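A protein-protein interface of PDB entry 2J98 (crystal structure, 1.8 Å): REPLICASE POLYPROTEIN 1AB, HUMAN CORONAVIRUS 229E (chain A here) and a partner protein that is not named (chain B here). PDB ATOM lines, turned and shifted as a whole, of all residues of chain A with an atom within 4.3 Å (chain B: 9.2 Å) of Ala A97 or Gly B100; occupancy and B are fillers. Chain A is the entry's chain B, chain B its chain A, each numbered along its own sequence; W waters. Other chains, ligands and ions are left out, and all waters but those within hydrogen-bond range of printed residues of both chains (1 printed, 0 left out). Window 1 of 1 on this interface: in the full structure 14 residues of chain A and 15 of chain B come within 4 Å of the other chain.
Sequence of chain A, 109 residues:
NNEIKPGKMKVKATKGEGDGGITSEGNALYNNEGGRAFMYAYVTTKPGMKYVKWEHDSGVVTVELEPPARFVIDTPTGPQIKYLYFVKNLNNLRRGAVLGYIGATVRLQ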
ATOM      1  N   PRO A   6      21.301  22.875  20.574  1.00  0.00           N
ATOM      2  CA  PRO A   6      22.497  22.421  19.826  1.00  0.00           C
ATOM      3  C   PRO A   6      23.257  23.576  19.177  1.00  0.00           C
ATOM      4  O   PRO A   6      24.460  23.459  18.933  1.00  0.00           O
ATOM      5  CB  PRO A   6      21.918  21.501  18.749  1.00  0.00           C
ATOM      6  CG  PRO A   6      20.613  21.030  19.314  1.00  0.00           C
ATOM      7  CD  PRO A   6      20.078  22.166  20.135  1.00  0.00           C
ATOM      8  N   GLY A   7      22.557  24.677  18.916  1.00  0.00           N
ATOM      9  CA  GLY A   7      23.138  25.865  18.289  1.00  0.00           C
ATOM     10  C   GLY A   7      24.220  26.583  19.094  1.00  0.00           C
ATOM     11  O   GLY A   7      25.141  27.137  18.513  1.00  0.00           O
ATOM     12  N   MET A   9      27.070  26.487  20.308  1.00  0.00           N
ATOM     13  CA  MET A   9      28.365  25.819  20.188  1.00  0.00           C
ATOM     14  C   MET A   9      29.495  26.675  20.730  1.00  0.00           C
ATOM     15  O   MET A   9      29.558  27.881  20.473  1.00  0.00           O
ATOM     16  CB  MET A   9      28.671  25.519  18.716  1.00  0.00           C
ATOM     17  CG  MET A   9      27.602  24.682  17.992  1.00  0.00           C
ATOM     18  SD  MET A   9      27.772  22.933  18.385  1.00  0.00           S
ATOM     19  CE  MET A   9      29.499  22.812  18.735  1.00  0.00           C
ATOM     20  N   LEU A  93      21.643  15.689  13.851  1.00  0.00           N
ATOM     21  CA  LEU A  93      21.393  17.054  14.338  1.00  0.00           C
ATOM     22  C   LEU A  93      22.677  17.710  14.833  1.00  0.00           C
ATOM     23  O   LEU A  93      22.985  18.854  14.476  1.00  0.00           O
ATOM     24  CB  LEU A  93      20.350  17.075  15.451  1.00  0.00           C
ATOM     25  CG  LEU A  93      19.816  18.460  15.835  1.00  0.00           C
ATOM     26  CD1 LEU A  93      19.027  19.026  14.669  1.00  0.00           C
ATOM     27  CD2 LEU A  93      18.884  18.323  17.045  1.00  0.00           C
ATOM     28  N   ARG A  94      23.448  16.961  15.631  1.00  0.00           N
ATOM     29  CA  ARG A  94      24.620  17.566  16.254  1.00  0.00           C
ATOM     30  C   ARG A  94      25.758  17.692  15.243  1.00  0.00           C
ATOM     31  O   ARG A  94      26.506  18.657  15.273  1.00  0.00           O
ATOM     32  CB  ARG A  94      25.060  16.813  17.508  1.00  0.00           C
ATOM     33  CG  ARG A  94      24.000  16.811  18.620  1.00  0.00           C
ATOM     34  CD  ARG A  94      24.426  15.936  19.827  1.00  0.00           C
ATOM     35  NE  ARG A  94      23.527  16.188  20.961  1.00  0.00           N
ATOM     36  CZ  ARG A  94      22.603  15.342  21.407  1.00  0.00           C
ATOM     37  NH1 ARG A  94      22.440  14.137  20.867  1.00  0.00           N
ATOM     38  NH2 ARG A  94      21.847  15.685  22.438  1.00  0.00           N
ATOM     39  N   ARG A  95      25.862  16.737  14.330  1.00  0.00           N
ATOM     40  CA  ARG A  95      26.801  16.887  13.209  1.00  0.00           C
ATOM     41  C   ARG A  95      26.530  18.121  12.399  1.00  0.00           C
ATOM     42  O   ARG A  95      27.496  18.856  12.082  1.00  0.00           O
ATOM     43  CB  ARG A  95      26.767  15.670  12.293  1.00  0.00           C
ATOM     44  CG  ARG A  95      27.326  14.410  12.966  1.00  0.00           C
ATOM     45  CD  ARG A  95      27.087  13.196  12.038  1.00  0.00           C
ATOM     46  NE  ARG A  95      27.466  12.007  12.797  1.00  0.00           N
ATOM     47  CZ  ARG A  95      28.592  11.332  12.615  1.00  0.00           C
ATOM     48  NH1 ARG A  95      28.860  10.282  13.383  1.00  0.00           N
ATOM     49  NH2 ARG A  95      29.442  11.703  11.670  1.00  0.00           N
ATOM     50  N   GLY A  96      25.235  18.377  12.100  1.00  0.00           N
ATOM     51  CA  GLY A  96      24.827  19.529  11.321  1.00  0.00           C
ATOM     52  C   GLY A  96      25.207  20.824  12.049  1.00  0.00           C
ATOM     53  O   GLY A  96      25.698  21.783  11.445  1.00  0.00           O
ATOM     54  N   ALA A  97      25.016  20.825  13.368  1.00  0.00           N
ATOM     55  CA  ALA A  97      25.353  22.016  14.175  1.00  0.00           C
ATOM     56  C   ALA A  97      26.850  22.312  14.053  1.00  0.00           C
ATOM     57  O   ALA A  97      27.254  23.481  13.915  1.00  0.00           O
ATOM     58  CB  ALA A  97      24.949  21.816  15.625  1.00  0.00           C
ATOM     59  N   VAL A  98      27.669  21.281  14.149  1.00  0.00           N
ATOM     60  CA  VAL A  98      29.122  21.459  13.881  1.00  0.00           C
ATOM     61  C   VAL A  98      29.352  22.071  12.490  1.00  0.00           C
ATOM     62  O   VAL A  98      30.046  23.062  12.371  1.00  0.00           O
ATOM     63  CB  VAL A  98      29.915  20.161  14.111  1.00  0.00           C
ATOM     64  CG1 VAL A  98      31.394  20.281  13.621  1.00  0.00           C
ATOM     65  CG2 VAL A  98      29.836  19.770  15.555  1.00  0.00           C
ATOM     66  N   LEU A  99      28.756  21.520  11.441  1.00  0.00           N
ATOM     67  CA  LEU A  99      29.048  22.011  10.074  1.00  0.00           C
ATOM     68  C   LEU A  99      28.588  23.463   9.886  1.00  0.00           C
ATOM     69  O   LEU A  99      29.268  24.293   9.250  1.00  0.00           O
ATOM     70  CB  LEU A  99      28.426  21.086   9.010  1.00  0.00           C
ATOM     71  CG  LEU A  99      28.787  19.605   9.079  1.00  0.00           C
ATOM     72  CD1 LEU A  99      27.918  18.823   8.093  1.00  0.00           C
ATOM     73  CD2 LEU A  99      30.211  19.461   8.778  1.00  0.00           C
ATOM     74  N   GLY A 100      27.440  23.782  10.457  1.00  0.00           N
ATOM     75  CA  GLY A 100      26.874  25.118  10.354  1.00  0.00           C
ATOM     76  C   GLY A 100      27.743  26.129  11.084  1.00  0.00           C
ATOM     77  O   GLY A 100      28.002  27.233  10.579  1.00  0.00           O
ATOM     78  N   TYR A 101      28.222  25.737  12.254  1.00  0.00           N
ATOM     79  CA  TYR A 101      29.097  26.606  13.073  1.00  0.00           C
ATOM     80  C   TYR A 101      30.393  26.827  12.322  1.00  0.00           C
ATOM     81  O   TYR A 101      30.865  27.958  12.216  1.00  0.00           O
ATOM     82  CB  TYR A 101      29.360  26.000  14.450  1.00  0.00           C
ATOM     83  CG  TYR A 101      30.470  26.711  15.207  1.00  0.00           C
ATOM     84  CD1 TYR A 101      30.217  27.773  16.071  1.00  0.00           C
ATOM     85  CD2 TYR A 101      31.779  26.287  15.036  1.00  0.00           C
ATOM     86  CE1 TYR A 101      31.290  28.417  16.761  1.00  0.00           C
ATOM     87  CE2 TYR A 101      32.839  26.920  15.691  1.00  0.00           C
ATOM     88  CZ  TYR A 101      32.585  27.971  16.532  1.00  0.00           C
ATOM     89  OH  TYR A 101      33.650  28.553  17.158  1.00  0.00           O
ATOM     90  N   ILE B   4      31.539  20.335   4.405  1.00  0.00           N
ATOM     91  CA  ILE B   4      30.819  21.452   5.020  1.00  0.00           C
ATOM     92  C   ILE B   4      29.702  22.002   4.104  1.00  0.00           C
ATOM     93  O   ILE B   4      28.967  22.904   4.503  1.00  0.00           O
ATOM     94  CB  ILE B   4      31.801  22.627   5.427  1.00  0.00           C
ATOM     95  CG1 ILE B   4      33.198  22.100   5.808  1.00  0.00           C
ATOM     96  CG2 ILE B   4      31.189  23.518   6.540  1.00  0.00           C
ATOM     97  CD1 ILE B   4      33.278  21.422   7.160  1.00  0.00           C
ATOM     98  N   PRO B   6      26.651  21.037   2.954  1.00  0.00           N
ATOM     99  CA  PRO B   6      25.247  21.127   3.428  1.00  0.00           C
ATOM    100  C   PRO B   6      25.042  22.053   4.634  1.00  0.00           C
ATOM    101  O   PRO B   6      23.901  22.399   4.958  1.00  0.00           O
ATOM    102  CB  PRO B   6      24.900  19.677   3.816  1.00  0.00           C
ATOM    103  CG  PRO B   6      26.207  19.031   4.109  1.00  0.00           C
ATOM    104  CD  PRO B   6      27.206  19.682   3.165  1.00  0.00           C
ATOM    105  N   GLY B   7      26.139  22.446   5.279  1.00  0.00           N
ATOM    106  CA  GLY B   7      26.089  23.366   6.408  1.00  0.00           C
ATOM    107  C   GLY B   7      26.315  24.825   6.029  1.00  0.00           C
ATOM    108  O   GLY B   7      26.088  25.718   6.846  1.00  0.00           O
ATOM    109  N   MET B   9      25.731  28.379   4.424  1.00  0.00           N
ATOM    110  CA  MET B   9      24.464  29.088   4.555  1.00  0.00           C
ATOM    111  C   MET B   9      24.563  30.562   4.268  1.00  0.00           C
ATOM    112  O   MET B   9      25.562  31.226   4.608  1.00  0.00           O
ATOM    113  CB  MET B   9      23.873  28.901   5.958  1.00  0.00           C
ATOM    114  CG  MET B   9      22.370  28.712   5.944  1.00  0.00           C
ATOM    115  SD  MET B   9      21.941  27.841   7.437  1.00  0.00           S
ATOM    116  CE  MET B   9      22.864  26.332   7.176  1.00  0.00           C
ATOM    117  N   LEU B  29      17.154  31.496   5.626  1.00  0.00           N
ATOM    118  CA  LEU B  29      18.467  30.920   5.650  1.00  0.00           C
ATOM    119  C   LEU B  29      18.471  29.831   4.572  1.00  0.00           C
ATOM    120  O   LEU B  29      17.587  29.000   4.521  1.00  0.00           O
ATOM    121  CB  LEU B  29      18.752  30.316   7.012  1.00  0.00           C
ATOM    122  CG  LEU B  29      18.919  31.410   8.083  1.00  0.00           C
ATOM    123  CD1 LEU B  29      18.776  30.866   9.496  1.00  0.00           C
ATOM    124  CD2 LEU B  29      20.291  31.995   7.877  1.00  0.00           C
ATOM    125  N   LEU B  84      12.038  30.548  15.084  1.00  0.00           N
ATOM    126  CA  LEU B  84      12.821  29.859  14.067  1.00  0.00           C
ATOM    127  C   LEU B  84      11.893  28.829  13.444  1.00  0.00           C
ATOM    128  O   LEU B  84      11.431  27.927  14.170  1.00  0.00           O
ATOM    129  CB  LEU B  84      13.982  29.137  14.762  1.00  0.00           C
ATOM    130  CG  LEU B  84      14.705  28.142  13.840  1.00  0.00           C
ATOM    131  CD1 LEU B  84      15.306  28.810  12.584  1.00  0.00           C
ATOM    132  CD2 LEU B  84      15.769  27.376  14.580  1.00  0.00           C
ATOM    133  N   PHE B  86      11.629  25.910  10.679  1.00  0.00           N
ATOM    134  CA  PHE B  86      12.234  25.101   9.627  1.00  0.00           C
ATOM    135  C   PHE B  86      11.274  24.908   8.461  1.00  0.00           C
ATOM    136  O   PHE B  86      10.076  24.889   8.655  1.00  0.00           O
ATOM    137  CB  PHE B  86      12.681  23.737  10.142  1.00  0.00           C
ATOM    138  CG  PHE B  86      13.789  23.830  11.158  1.00  0.00           C
ATOM    139  CD1 PHE B  86      13.566  23.453  12.485  1.00  0.00           C
ATOM    140  CD2 PHE B  86      15.046  24.311  10.805  1.00  0.00           C
ATOM    141  CE1 PHE B  86      14.607  23.525  13.440  1.00  0.00           C
ATOM    142  CE2 PHE B  86      16.089  24.395  11.764  1.00  0.00           C
ATOM    143  CZ  PHE B  86      15.860  24.007  13.070  1.00  0.00           C
ATOM    144  N   ASN B  92      17.443  16.250   9.569  1.00  0.00           N
ATOM    145  CA  ASN B  92      18.108  16.638  10.818  1.00  0.00           C
ATOM    146  C   ASN B  92      19.478  17.272  10.598  1.00  0.00           C
ATOM    147  O   ASN B  92      19.882  18.149  11.352  1.00  0.00           O
ATOM    148  CB  ASN B  92      18.196  15.435  11.768  1.00  0.00           C
ATOM    149  CG  ASN B  92      16.849  15.136  12.428  1.00  0.00           C
ATOM    150  OD1 ASN B  92      16.064  16.051  12.682  1.00  0.00           O
ATOM    151  ND2 ASN B  92      16.575  13.897  12.673  1.00  0.00           N
ATOM    152  N   LEU B  93      20.208  16.783   9.607  1.00  0.00           N
ATOM    153  CA  LEU B  93      21.541  17.356   9.315  1.00  0.00           C
ATOM    154  C   LEU B  93      21.396  18.838   8.996  1.00  0.00           C
ATOM    155  O   LEU B  93      22.120  19.672   9.556  1.00  0.00           O
ATOM    156  CB  LEU B  93      22.192  16.641   8.134  1.00  0.00           C
ATOM    157  CG  LEU B  93      23.575  17.174   7.721  1.00  0.00           C
ATOM    158  CD1 LEU B  93      24.518  16.737   8.799  1.00  0.00           C
ATOM    159  CD2 LEU B  93      23.964  16.584   6.407  1.00  0.00           C
ATOM    160  N   ARG B  94      20.415  19.182   8.154  1.00  0.00           N
ATOM    161  CA  ARG B  94      20.196  20.566   7.764  1.00  0.00           C
ATOM    162  C   ARG B  94      19.597  21.427   8.867  1.00  0.00           C
ATOM    163  O   ARG B  94      19.927  22.595   8.975  1.00  0.00           O
ATOM    164  CB  ARG B  94      19.388  20.690   6.460  1.00  0.00           C
ATOM    165  CG  ARG B  94      20.189  20.134   5.289  1.00  0.00           C
ATOM    166  CD  ARG B  94      19.369  19.997   4.026  1.00  0.00           C
ATOM    167  NE  ARG B  94      20.271  19.852   2.892  1.00  0.00           N
ATOM    168  CZ  ARG B  94      20.886  18.728   2.541  1.00  0.00           C
ATOM    169  NH1 ARG B  94      21.706  18.744   1.503  1.00  0.00           N
ATOM    170  NH2 ARG B  94      20.694  17.587   3.215  1.00  0.00           N
ATOM    171  N   ARG B  95      18.720  20.860   9.687  1.00  0.00           N
ATOM    172  CA  ARG B  95      18.215  21.600  10.841  1.00  0.00           C
ATOM    173  C   ARG B  95      19.388  21.961  11.744  1.00  0.00           C
ATOM    174  O   ARG B  95      19.492  23.085  12.214  1.00  0.00           O
ATOM    175  CB  ARG B  95      17.290  20.677  11.648  1.00  0.00           C
ATOM    176  CG  ARG B  95      15.933  20.599  11.023  1.00  0.00           C
ATOM    177  CD  ARG B  95      15.056  19.644  11.818  1.00  0.00           C
ATOM    178  NE  ARG B  95      13.990  19.284  10.884  1.00  0.00           N
ATOM    179  CZ  ARG B  95      12.710  19.529  11.089  1.00  0.00           C
ATOM    180  NH1 ARG B  95      12.322  20.076  12.251  1.00  0.00           N
ATOM    181  NH2 ARG B  95      11.838  19.211  10.129  1.00  0.00           N
ATOM    182  N   GLY B  96      20.282  20.994  11.946  1.00  0.00           N
ATOM    183  CA  GLY B  96      21.479  21.185  12.786  1.00  0.00           C
ATOM    184  C   GLY B  96      22.342  22.292  12.207  1.00  0.00           C
ATOM    185  O   GLY B  96      22.807  23.164  12.910  1.00  0.00           O
ATOM    186  N   ALA B  97      22.515  22.269  10.898  1.00  0.00           N
ATOM    187  CA  ALA B  97      23.298  23.294  10.237  1.00  0.00           C
ATOM    188  C   ALA B  97      22.726  24.703  10.480  1.00  0.00           C
ATOM    189  O   ALA B  97      23.466  25.669  10.800  1.00  0.00           O
ATOM    190  CB  ALA B  97      23.397  22.956   8.756  1.00  0.00           C
ATOM    191  N   VAL B  98      21.402  24.823  10.394  1.00  0.00           N
ATOM    192  CA  VAL B  98      20.735  26.064  10.719  1.00  0.00           C
ATOM    193  C   VAL B  98      21.049  26.505  12.164  1.00  0.00           C
ATOM    194  O   VAL B  98      21.464  27.657  12.391  1.00  0.00           O
ATOM    195  CB  VAL B  98      19.240  25.948  10.506  1.00  0.00           C
ATOM    196  CG1 VAL B  98      18.492  27.101  11.254  1.00  0.00           C
ATOM    197  CG2 VAL B  98      18.915  25.899   9.019  1.00  0.00           C
ATOM    198  N   LEU B  99      20.889  25.601  13.136  1.00  0.00           N
ATOM    199  CA  LEU B  99      21.187  25.925  14.542  1.00  0.00           C
ATOM    200  C   LEU B  99      22.649  26.359  14.768  1.00  0.00           C
ATOM    201  O   LEU B  99      22.922  27.349  15.493  1.00  0.00           O
ATOM    202  CB  LEU B  99      20.839  24.699  15.419  1.00  0.00           C
ATOM    203  CG  LEU B  99      19.349  24.350  15.443  1.00  0.00           C
ATOM    204  CD1 LEU B  99      19.166  23.050  16.193  1.00  0.00           C
ATOM    205  CD2 LEU B  99      18.512  25.469  16.064  1.00  0.00           C
ATOM    206  N   GLY B 100      23.584  25.652  14.122  1.00  0.00           N
ATOM    207  CA  GLY B 100      25.024  25.964  14.229  1.00  0.00           C
ATOM    208  C   GLY B 100      25.326  27.340  13.654  1.00  0.00           C
ATOM    209  O   GLY B 100      26.124  28.107  14.201  1.00  0.00           O
ATOM    210  N   TYR B 101      24.687  27.647  12.519  1.00  0.00           N
ATOM    211  CA  TYR B 101      24.911  28.939  11.853  1.00  0.00           C
ATOM    212  C   TYR B 101      24.348  30.073  12.714  1.00  0.00           C
ATOM    213  O   TYR B 101      25.015  31.096  12.954  1.00  0.00           O
ATOM    214  CB  TYR B 101      24.277  28.925  10.469  1.00  0.00           C
ATOM    215  CG  TYR B 101      24.202  30.325   9.851  1.00  0.00           C
ATOM    216  CD1 TYR B 101      25.202  30.787   8.996  1.00  0.00           C
ATOM    217  CD2 TYR B 101      23.154  31.162  10.168  1.00  0.00           C
ATOM    218  CE1 TYR B 101      25.126  32.092   8.479  1.00  0.00           C
ATOM    219  CE2 TYR B 101      23.075  32.449   9.670  1.00  0.00           C
ATOM    220  CZ  TYR B 101      24.043  32.891   8.830  1.00  0.00           C
ATOM    221  OH  TYR B 101      23.919  34.184   8.363  1.00  0.00           O
ATOM    222  N   ILE B 102      23.164  29.867  13.247  1.00  0.00           N
ATOM    223  CA  ILE B 102      22.590  30.890  14.109  1.00  0.00           C
ATOM    224  C   ILE B 102      23.470  31.098  15.353  1.00  0.00           C
ATOM    225  O   ILE B 102      23.803  32.250  15.705  1.00  0.00           O
ATOM    226  CB  ILE B 102      21.152  30.532  14.479  1.00  0.00           C
ATOM    227  CG1 ILE B 102      20.270  30.722  13.258  1.00  0.00           C
ATOM    228  CG2 ILE B 102      20.666  31.426  15.653  1.00  0.00           C
ATOM    229  CD1 ILE B 102      18.852  30.100  13.452  1.00  0.00           C
ATOM    230  N   GLY B 103      23.870  30.005  15.984  1.00  0.00           N
ATOM    231  CA  GLY B 103      24.731  30.055  17.159  1.00  0.00           C
ATOM    232  C   GLY B 103      26.029  30.835  16.895  1.00  0.00           C
ATOM    233  O   GLY B 103      26.482  31.617  17.737  1.00  0.00           O
ATOM    234  N   ALA B 104      26.612  30.631  15.719  1.00  0.00           N
ATOM    235  CA  ALA B 104      27.883  31.260  15.341  1.00  0.00           C
ATOM    236  C   ALA B 104      27.758  32.744  15.037  1.00  0.00           C
ATOM    237  O   ALA B 104      28.745  33.480  15.103  1.00  0.00           O
ATOM    238  CB  ALA B 104      28.497  30.532  14.121  1.00  0.00           C
ATOM    239  N   THR B 105      26.568  33.196  14.670  1.00  0.00           N
ATOM    240  CA  THR B 105      26.439  34.527  14.095  1.00  0.00           C
ATOM    241  C   THR B 105      25.577  35.454  14.952  1.00  0.00           C
ATOM    242  O   THR B 105      25.720  36.672  14.897  1.00  0.00           O
ATOM    243  CB  THR B 105      25.855  34.479  12.643  1.00  0.00           C
ATOM    244  OG1 THR B 105      24.598  33.861  12.672  1.00  0.00           O
ATOM    245  CG2 THR B 105      26.744  33.687  11.735  1.00  0.00           C
ATOM    246  N   VAL B 106      24.684  34.869  15.741  1.00  0.00           N
ATOM    247  CA  VAL B 106      23.768  35.652  16.593  1.00  0.00           C
ATOM    248  C   VAL B 106      24.279  35.666  18.039  1.00  0.00           C
ATOM    249  O   VAL B 106      24.927  34.727  18.468  1.00  0.00           O
ATOM    250  CB  VAL B 106      22.316  35.037  16.487  1.00  0.00           C
ATOM    251  CG1 VAL B 106      21.510  35.256  17.733  1.00  0.00           C
ATOM    252  CG2 VAL B 106      21.597  35.576  15.231  1.00  0.00           C
ATOM    253  N   LEU B 108      23.198  34.864  21.285  1.00  0.00           N
ATOM    254  CA  LEU B 108      22.067  34.114  21.855  1.00  0.00           C
ATOM    255  C   LEU B 108      21.870  34.371  23.342  1.00  0.00           C
ATOM    256  O   LEU B 108      22.844  34.549  24.082  1.00  0.00           O
ATOM    257  CB  LEU B 108      22.233  32.610  21.605  1.00  0.00           C
ATOM    258  CG  LEU B 108      21.901  32.071  20.213  1.00  0.00           C
ATOM    259  CD1 LEU B 108      22.300  30.610  20.089  1.00  0.00           C
ATOM    260  CD2 LEU B 108      20.417  32.241  19.901  1.00  0.00           C
HETATM  261  O   HOH W   1      26.901  27.957   7.929  1.00  0.00           O
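O of Gly B96 sits close to N of Ala A97 (3.2 Å). The backbone NH (N) of Ala B97 lies close to the backbone carbonyl oxygen (O) of Gly A96, at 3.3 Å.
O of Tyr B101 sits at hydrogen-bond distance from OG1 of Thr B105, at 2.8 Å.
Pro A6 touches Leu B99. O of Leu B99 touches CA of Gly A7, 3.2 Å away. O of Asn B92 touches CA of Leu A93, at 3.5 Å. O of Leu B93 touches CA of Gly A96, 3.2 Å away. Gly A96 touches Gly B96. Ala B97 touches Ala A97 (N to N, 3.8 Å). Ala A97 touches Gly B100 (O to CA, 3.4 Å). Gly A100 touches Gly B100 (C to C, 3.7 Å). CA of Tyr A101 touches O of Gly B100, at 3.5 Å. CB of Ala B104 touches CD1 of Tyr A101, 3.8 Å away.
Of chain B, only Leu B93, Gly B96 and Ala B97 come within 4 Å of Gly A96. Of chain B, only Gly B96 (3.1 Å), Ala B97 (3.8 Å) and Gly B100 (3.4 Å) come within 4 Å of Ala A97. Val A98 touches none of the printed residues of chain B. Gly A100 touches just these residues of chain B: Gly B7 (3.6 Å), Ala B97 (3.5 Å), Gly B100 (3.7 Å) and Tyr B101 (3.7 Å). Printed residues of chain A within 4 Å of Ile B4: Leu A99 (3.4 Å). Of the printed residues of chain A, Asn B92 touches Leu A93. Of the printed residues of chain A, Arg B95 touches Leu A93 (3.9 Å). Val B98 touches none of the printed residues of chain A. Printed residues of chain A within 4 Å of Tyr B101: Gly A100 (3.7 Å). Printed residues of chain A within 4 Å of Ala B104: Tyr A101.
Printed residues of chain B that touch a printed residue of chain A: Ile B4, Gly B7, Asn B92, Leu B93, Arg B95, Gly B96, Ala B97, Leu B99, Gly B100, Tyr B101, Gly B103 and Ala B104. Hydrophobic or aromatic side chains of chain B that line the printed part of chain A: Ile B4, Leu B93, Ala B97, Leu B99 and Ala B104. Printed residues of chain A that touch a printed residue of chain B: Pro A6, Gly A7, Leu A93, Gly A96, Ala A97, Leu A99, Gly A100 and Tyr A101. Among the printed residues, 19 pairs touch across the chains. Among the printed residues, no Asp or Glu carboxylate lies within 4 Å of a Lys or Arg side-chain nitrogen of the other chain.
Water W1 bridges the backbone carbonyl oxygen (O) of Gly B7 (2.6 Å) and the backbone carbonyl oxygen (O) of Gly A100 (3.0 Å).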
